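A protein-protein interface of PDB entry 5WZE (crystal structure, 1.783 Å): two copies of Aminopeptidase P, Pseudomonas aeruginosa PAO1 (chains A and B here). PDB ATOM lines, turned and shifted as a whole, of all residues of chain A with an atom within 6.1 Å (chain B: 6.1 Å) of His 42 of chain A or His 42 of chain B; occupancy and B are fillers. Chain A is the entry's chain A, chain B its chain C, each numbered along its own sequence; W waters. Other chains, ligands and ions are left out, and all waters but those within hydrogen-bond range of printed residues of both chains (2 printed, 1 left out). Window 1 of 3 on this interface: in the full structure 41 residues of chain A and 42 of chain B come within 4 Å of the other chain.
Tyr 34 of chain A touches its own counterpart, Tyr 34 of chain B. Tyr 34 of chain A touches Ile 35 of chain B, and with the chains exchanged Ile 35 of chain A touches Tyr 34 of chain B. Tyr 34 of chain A touches His 42 of chain B, and with the chains exchanged His 42 of chain A touches Tyr 34 of chain B. His 42 of chain A touches its own counterpart, His 42 of chain B. 9 positions are printed for both chains.
The backbone carbonyl oxygen (O) of Tyr 34 of chain A sits at hydrogen-bond distance from the backbone NH (N) of His 42 of chain A, at 3.0 Å. The backbone carbonyl oxygen of Tyr 34 of chain B is in hydrogen-bond range of the backbone NH of His 42 of chain B, 2.9 Å away.
Hydrophobic or aromatic side chains of chain A within 4 Å of the printed part of chain B: Tyr 34 and His 42. Along chain B the printed residues that touch a printed residue of chain A span positions 34 to 45. Among the printed residues, 10 pairs touch across the chains.
A ring nitrogen (NE2) of His 42 of chain B lies within hydrogen-bond range of the backbone carbonyl oxygen (O) of Val 43 of chain A, 3.3 Å away.
Printed residues of chain B within 4 Å of Tyr 34 of chain A: Tyr 34 (3.5 Å), Ile 35 (3.5 Å) and His 42 (3.7 Å). Of the printed residues of chain B, Ile 35 of chain A touches Tyr 34 (3.6 Å). Of the printed residues of chain B, Arg 36 of chain A touches Arg 45. Of chain B, only Tyr 34 (3.97 Å), His 42 (3.6 Å) and Val 43 (3.2 Å) come within 4 Å of His 42 of chain A. Of the printed residues of chain B, Arg 45 of chain A touches Arg 36. Printed residues of chain A within 4 Å of Ile 35 of chain B: Tyr 34 (3.5 Å). Of chain A, only Tyr 34, His 42 and Val 43 come within 4 Å of His 42 of chain B. Tyr 44 of chain B touches none of the printed residues of chain A.
CD1 of Tyr 34 of chain B touches CD1 of Tyr 34 of chain A, at 3.5 Å. CE2 of Tyr 34 of chain A touches O of Ile 35 of chain B, at 3.5 Å. Tyr 34 of chain A touches His 42 of chain B. CE2 of Tyr 34 of chain B touches O of Ile 35 of chain A, at 3.6 Å. Arg 36 of chain A touches Arg 45 of chain B (CG to CB, 3.9 Å). His 42 of chain A touches Tyr 34 of chain B (NE2 to CD2, 3.97 Å). His 42 of chain A touches His 42 of chain B (ND1 to CD2, 3.6 Å). CE1 of His 42 of chain A touches O of Val 43 of chain B, 3.2 Å away. Arg 36 of chain B touches Arg 45 of chain A (CG to CB, 3.9 Å).
Water W1 lies within hydrogen-bond range of O of Arg 36 of chain A (2.6 Å) and O of Arg 45 of chain B (3.0 Å). Water W2 bridges O of Arg 36 of chain B and O of Arg 45 of chain A.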
ATOM      1  N   TYR A  34     -19.176 -18.988 -24.303  1.00  0.00           N
ATOM      2  CA  TYR A  34     -20.015 -17.877 -24.723  1.00  0.00           C
ATOM      3  C   TYR A  34     -19.325 -17.059 -25.802  1.00  0.00           C
ATOM      4  O   TYR A  34     -18.114 -16.844 -25.748  1.00  0.00           O
ATOM      5  CB  TYR A  34     -20.358 -16.966 -23.545  1.00  0.00           C
ATOM      6  CG  TYR A  34     -21.019 -17.673 -22.395  1.00  0.00           C
ATOM      7  CD1 TYR A  34     -22.339 -18.080 -22.475  1.00  0.00           C
ATOM      8  CD2 TYR A  34     -20.324 -17.923 -21.222  1.00  0.00           C
ATOM      9  CE1 TYR A  34     -22.948 -18.721 -21.420  1.00  0.00           C
ATOM     10  CE2 TYR A  34     -20.926 -18.562 -20.165  1.00  0.00           C
ATOM     11  CZ  TYR A  34     -22.234 -18.956 -20.268  1.00  0.00           C
ATOM     12  OH  TYR A  34     -22.828 -19.592 -19.207  1.00  0.00           O
ATOM     13  N   ILE A  35     -20.102 -16.584 -26.767  1.00  0.00           N
ATOM     14  CA  ILE A  35     -19.607 -15.644 -27.767  1.00  0.00           C
ATOM     15  C   ILE A  35     -19.796 -14.225 -27.247  1.00  0.00           C
ATOM     16  O   ILE A  35     -20.884 -13.868 -26.794  1.00  0.00           O
ATOM     17  CB  ILE A  35     -20.331 -15.831 -29.108  1.00  0.00           C
ATOM     18  CG1 ILE A  35     -19.919 -17.144 -29.756  1.00  0.00           C
ATOM     19  CG2 ILE A  35     -20.023 -14.677 -30.023  1.00  0.00           C
ATOM     20  CD1 ILE A  35     -18.465 -17.212 -30.095  1.00  0.00           C
ATOM     21  N   ARG A  36     -18.734 -13.417 -27.303  1.00  0.00           N
ATOM     22  CA  ARG A  36     -18.822 -12.046 -26.822  1.00  0.00           C
ATOM     23  C   ARG A  36     -19.417 -11.134 -27.888  1.00  0.00           C
ATOM     24  O   ARG A  36     -20.341 -10.364 -27.609  1.00  0.00           O
ATOM     25  CB  ARG A  36     -17.437 -11.545 -26.389  1.00  0.00           C
ATOM     26  CG  ARG A  36     -17.443 -10.225 -25.639  1.00  0.00           C
ATOM     27  CD  ARG A  36     -16.039  -9.642 -25.504  1.00  0.00           C
ATOM     28  NE  ARG A  36     -15.583  -9.045 -26.747  1.00  0.00           N
ATOM     29  CZ  ARG A  36     -14.416  -8.437 -26.906  1.00  0.00           C
ATOM     30  NH1 ARG A  36     -13.562  -8.341 -25.899  1.00  0.00           N
ATOM     31  NH2 ARG A  36     -14.112  -7.919 -28.079  1.00  0.00           N
ATOM     32  N   VAL A  40     -15.899 -13.588 -31.678  1.00  0.00           N
ATOM     33  CA  VAL A  40     -14.974 -13.379 -30.577  1.00  0.00           C
ATOM     34  C   VAL A  40     -15.590 -13.983 -29.328  1.00  0.00           C
ATOM     35  O   VAL A  40     -16.676 -13.582 -28.912  1.00  0.00           O
ATOM     36  CB  VAL A  40     -14.687 -11.886 -30.378  1.00  0.00           C
ATOM     37  CG1 VAL A  40     -13.764 -11.678 -29.199  1.00  0.00           C
ATOM     38  CG2 VAL A  40     -14.086 -11.306 -31.617  1.00  0.00           C
ATOM     39  N   GLU A  41     -14.903 -14.937 -28.723  1.00  0.00           N
ATOM     40  CA  GLU A  41     -15.455 -15.580 -27.544  1.00  0.00           C
ATOM     41  C   GLU A  41     -14.999 -14.877 -26.271  1.00  0.00           C
ATOM     42  O   GLU A  41     -13.958 -14.215 -26.233  1.00  0.00           O
ATOM     43  CB  GLU A  41     -15.079 -17.059 -27.498  1.00  0.00           C
ATOM     44  CG  GLU A  41     -13.646 -17.351 -27.843  1.00  0.00           C
ATOM     45  CD  GLU A  41     -13.345 -18.837 -27.920  1.00  0.00           C
ATOM     46  OE1 GLU A  41     -13.911 -19.528 -28.793  1.00  0.00           O
ATOM     47  OE2 GLU A  41     -12.535 -19.315 -27.100  1.00  0.00           O
ATOM     48  N   HIS A  42     -15.820 -14.997 -25.238  1.00  0.00           N
ATOM     49  CA  HIS A  42     -15.459 -14.542 -23.911  1.00  0.00           C
ATOM     50  C   HIS A  42     -14.331 -15.401 -23.367  1.00  0.00           C
ATOM     51  O   HIS A  42     -14.147 -16.552 -23.767  1.00  0.00           O
ATOM     52  CB  HIS A  42     -16.659 -14.634 -22.964  1.00  0.00           C
ATOM     53  CG  HIS A  42     -17.508 -13.405 -22.914  1.00  0.00           C
ATOM     54  ND1 HIS A  42     -17.031 -12.189 -22.484  1.00  0.00           N
ATOM     55  CD2 HIS A  42     -18.821 -13.216 -23.192  1.00  0.00           C
ATOM     56  CE1 HIS A  42     -18.003 -11.299 -22.516  1.00  0.00           C
ATOM     57  NE2 HIS A  42     -19.103 -11.898 -22.933  1.00  0.00           N
ATOM     58  N   VAL A  43     -13.586 -14.844 -22.419  1.00  0.00           N
ATOM     59  CA  VAL A  43     -12.573 -15.644 -21.752  1.00  0.00           C
ATOM     60  C   VAL A  43     -13.256 -16.834 -21.097  1.00  0.00           C
ATOM     61  O   VAL A  43     -14.350 -16.705 -20.546  1.00  0.00           O
ATOM     62  CB  VAL A  43     -11.792 -14.785 -20.746  1.00  0.00           C
ATOM     63  CG1 VAL A  43     -12.714 -14.216 -19.665  1.00  0.00           C
ATOM     64  CG2 VAL A  43     -10.649 -15.572 -20.145  1.00  0.00           C
ATOM     65  N   TYR A  44     -12.655 -18.016 -21.227  1.00  0.00           N
ATOM     66  CA  TYR A  44     -13.264 -19.226 -20.687  1.00  0.00           C
ATOM     67  C   TYR A  44     -13.030 -19.326 -19.188  1.00  0.00           C
ATOM     68  O   TYR A  44     -11.940 -19.027 -18.698  1.00  0.00           O
ATOM     69  CB  TYR A  44     -12.721 -20.488 -21.369  1.00  0.00           C
ATOM     70  CG  TYR A  44     -13.481 -21.722 -20.938  1.00  0.00           C
ATOM     71  CD1 TYR A  44     -14.817 -21.862 -21.241  1.00  0.00           C
ATOM     72  CD2 TYR A  44     -12.890 -22.703 -20.183  1.00  0.00           C
ATOM     73  CE1 TYR A  44     -15.533 -22.958 -20.832  1.00  0.00           C
ATOM     74  CE2 TYR A  44     -13.599 -23.813 -19.778  1.00  0.00           C
ATOM     75  CZ  TYR A  44     -14.921 -23.926 -20.103  1.00  0.00           C
ATOM     76  OH  TYR A  44     -15.639 -25.010 -19.696  1.00  0.00           O
ATOM     77  N   ARG A  45     -14.057 -19.758 -18.454  1.00  0.00           N
ATOM     78  CA  ARG A  45     -13.952 -19.992 -17.018  1.00  0.00           C
ATOM     79  C   ARG A  45     -14.613 -21.315 -16.681  1.00  0.00           C
ATOM     80  O   ARG A  45     -15.825 -21.452 -16.826  1.00  0.00           O
ATOM     81  CB  ARG A  45     -14.603 -18.872 -16.199  1.00  0.00           C
ATOM     82  CG  ARG A  45     -14.725 -19.182 -14.692  1.00  0.00           C
ATOM     83  CD  ARG A  45     -13.381 -19.529 -14.045  1.00  0.00           C
ATOM     84  NE  ARG A  45     -13.253 -19.047 -12.670  1.00  0.00           N
ATOM     85  CZ  ARG A  45     -13.775 -19.654 -11.608  1.00  0.00           C
ATOM     86  NH1 ARG A  45     -14.478 -20.759 -11.749  1.00  0.00           N
ATOM     87  NH2 ARG A  45     -13.611 -19.151 -10.401  1.00  0.00           N
ATOM     88  N   TYR B  34     -24.260 -12.397 -19.815  1.00  0.00           N
ATOM     89  CA  TYR B  34     -23.866 -13.757 -19.496  1.00  0.00           C
ATOM     90  C   TYR B  34     -23.282 -13.824 -18.092  1.00  0.00           C
ATOM     91  O   TYR B  34     -22.565 -12.917 -17.660  1.00  0.00           O
ATOM     92  CB  TYR B  34     -22.838 -14.286 -20.504  1.00  0.00           C
ATOM     93  CG  TYR B  34     -23.310 -14.258 -21.933  1.00  0.00           C
ATOM     94  CD1 TYR B  34     -24.267 -15.152 -22.384  1.00  0.00           C
ATOM     95  CD2 TYR B  34     -22.796 -13.344 -22.833  1.00  0.00           C
ATOM     96  CE1 TYR B  34     -24.703 -15.128 -23.693  1.00  0.00           C
ATOM     97  CE2 TYR B  34     -23.225 -13.312 -24.143  1.00  0.00           C
ATOM     98  CZ  TYR B  34     -24.174 -14.207 -24.567  1.00  0.00           C
ATOM     99  OH  TYR B  34     -24.597 -14.174 -25.872  1.00  0.00           O
ATOM    100  N   ILE B  35     -23.583 -14.908 -17.400  1.00  0.00           N
ATOM    101  CA  ILE B  35     -22.947 -15.241 -16.135  1.00  0.00           C
ATOM    102  C   ILE B  35     -21.646 -15.985 -16.403  1.00  0.00           C
ATOM    103  O   ILE B  35     -21.633 -16.995 -17.118  1.00  0.00           O
ATOM    104  CB  ILE B  35     -23.874 -16.096 -15.262  1.00  0.00           C
ATOM    105  CG1 ILE B  35     -25.062 -15.280 -14.790  1.00  0.00           C
ATOM    106  CG2 ILE B  35     -23.094 -16.656 -14.089  1.00  0.00           C
ATOM    107  CD1 ILE B  35     -24.655 -14.105 -13.979  1.00  0.00           C
ATOM    108  N   ARG B  36     -20.560 -15.509 -15.795  1.00  0.00           N
ATOM    109  CA  ARG B  36     -19.264 -16.163 -15.923  1.00  0.00           C
ATOM    110  C   ARG B  36     -19.139 -17.351 -14.972  1.00  0.00           C
ATOM    111  O   ARG B  36     -18.738 -18.445 -15.383  1.00  0.00           O
ATOM    112  CB  ARG B  36     -18.144 -15.150 -15.661  1.00  0.00           C
ATOM    113  CG  ARG B  36     -16.777 -15.591 -16.118  1.00  0.00           C
ATOM    114  CD  ARG B  36     -15.679 -14.710 -15.543  1.00  0.00           C
ATOM    115  NE  ARG B  36     -15.464 -14.995 -14.135  1.00  0.00           N
ATOM    116  CZ  ARG B  36     -14.558 -14.392 -13.377  1.00  0.00           C
ATOM    117  NH1 ARG B  36     -13.773 -13.452 -13.893  1.00  0.00           N
ATOM    118  NH2 ARG B  36     -14.437 -14.733 -12.103  1.00  0.00           N
ATOM    119  N   VAL B  40     -21.221 -14.070 -10.804  1.00  0.00           N
ATOM    120  CA  VAL B  40     -20.305 -13.097 -11.379  1.00  0.00           C
ATOM    121  C   VAL B  40     -20.607 -12.980 -12.863  1.00  0.00           C
ATOM    122  O   VAL B  40     -20.612 -13.980 -13.588  1.00  0.00           O
ATOM    123  CB  VAL B  40     -18.845 -13.504 -11.150  1.00  0.00           C
ATOM    124  CG1 VAL B  40     -17.910 -12.499 -11.798  1.00  0.00           C
ATOM    125  CG2 VAL B  40     -18.564 -13.647  -9.660  1.00  0.00           C
ATOM    126  N   GLU B  41     -20.860 -11.764 -13.322  1.00  0.00           N
ATOM    127  CA  GLU B  41     -21.170 -11.508 -14.717  1.00  0.00           C
ATOM    128  C   GLU B  41     -19.899 -11.392 -15.543  1.00  0.00           C
ATOM    129  O   GLU B  41     -18.850 -10.991 -15.044  1.00  0.00           O
ATOM    130  CB  GLU B  41     -21.972 -10.218 -14.866  1.00  0.00           C
ATOM    131  CG  GLU B  41     -23.191 -10.125 -13.981  1.00  0.00           C
ATOM    132  CD  GLU B  41     -23.848  -8.767 -14.081  1.00  0.00           C
ATOM    133  OE1 GLU B  41     -24.997  -8.620 -13.619  1.00  0.00           O
ATOM    134  OE2 GLU B  41     -23.209  -7.840 -14.620  1.00  0.00           O
ATOM    135  N   HIS B  42     -20.005 -11.764 -16.812  1.00  0.00           N
ATOM    136  CA  HIS B  42     -19.012 -11.410 -17.805  1.00  0.00           C
ATOM    137  C   HIS B  42     -19.088  -9.921 -18.102  1.00  0.00           C
ATOM    138  O   HIS B  42     -20.141  -9.296 -17.973  1.00  0.00           O
ATOM    139  CB  HIS B  42     -19.241 -12.200 -19.097  1.00  0.00           C
ATOM    140  CG  HIS B  42     -18.424 -13.446 -19.205  1.00  0.00           C
ATOM    141  ND1 HIS B  42     -18.985 -14.686 -19.410  1.00  0.00           N
ATOM    142  CD2 HIS B  42     -17.088 -13.644 -19.149  1.00  0.00           C
ATOM    143  CE1 HIS B  42     -18.031 -15.595 -19.462  1.00  0.00           C
ATOM    144  NE2 HIS B  42     -16.871 -14.989 -19.309  1.00  0.00           N
ATOM    145  N   VAL B  43     -17.952  -9.350 -18.507  1.00  0.00           N
ATOM    146  CA  VAL B  43     -17.950  -7.969 -18.972  1.00  0.00           C
ATOM    147  C   VAL B  43     -18.973  -7.813 -20.087  1.00  0.00           C
ATOM    148  O   VAL B  43     -19.119  -8.683 -20.953  1.00  0.00           O
ATOM    149  CB  VAL B  43     -16.551  -7.547 -19.444  1.00  0.00           C
ATOM    150  CG1 VAL B  43     -16.146  -8.344 -20.677  1.00  0.00           C
ATOM    151  CG2 VAL B  43     -16.527  -6.064 -19.747  1.00  0.00           C
ATOM    152  N   TYR B  44     -19.717  -6.716 -20.054  1.00  0.00           N
ATOM    153  CA  TYR B  44     -20.787  -6.533 -21.020  1.00  0.00           C
ATOM    154  C   TYR B  44     -20.254  -5.912 -22.295  1.00  0.00           C
ATOM    155  O   TYR B  44     -19.505  -4.938 -22.261  1.00  0.00           O
ATOM    156  CB  TYR B  44     -21.898  -5.643 -20.468  1.00  0.00           C
ATOM    157  CG  TYR B  44     -23.062  -5.543 -21.432  1.00  0.00           C
ATOM    158  CD1 TYR B  44     -23.870  -6.640 -21.688  1.00  0.00           C
ATOM    159  CD2 TYR B  44     -23.350  -4.360 -22.089  1.00  0.00           C
ATOM    160  CE1 TYR B  44     -24.937  -6.556 -22.569  1.00  0.00           C
ATOM    161  CE2 TYR B  44     -24.420  -4.267 -22.972  1.00  0.00           C
ATOM    162  CZ  TYR B  44     -25.207  -5.364 -23.204  1.00  0.00           C
ATOM    163  OH  TYR B  44     -26.255  -5.273 -24.090  1.00  0.00           O
ATOM    164  N   ARG B  45     -20.677  -6.455 -23.425  1.00  0.00           N
ATOM    165  CA  ARG B  45     -20.319  -5.904 -24.720  1.00  0.00           C
ATOM    166  C   ARG B  45     -21.591  -5.744 -25.537  1.00  0.00           C
ATOM    167  O   ARG B  45     -22.288  -6.726 -25.802  1.00  0.00           O
ATOM    168  CB  ARG B  45     -19.300  -6.803 -25.427  1.00  0.00           C
ATOM    169  CG  ARG B  45     -19.009  -6.438 -26.862  1.00  0.00           C
ATOM    170  CD  ARG B  45     -18.551  -4.998 -27.027  1.00  0.00           C
ATOM    171  NE  ARG B  45     -17.598  -4.848 -28.125  1.00  0.00           N
ATOM    172  CZ  ARG B  45     -17.923  -4.755 -29.408  1.00  0.00           C
ATOM    173  NH1 ARG B  45     -19.191  -4.793 -29.783  1.00  0.00           N
ATOM    174  NH2 ARG B  45     -16.976  -4.633 -30.319  1.00  0.00           N
HETATM  175  O   HOH W   1     -21.992  -8.439 -28.302  1.00  0.00           O
HETATM  176  O   HOH W   2     -18.137 -21.002 -14.933  1.00  0.00           O
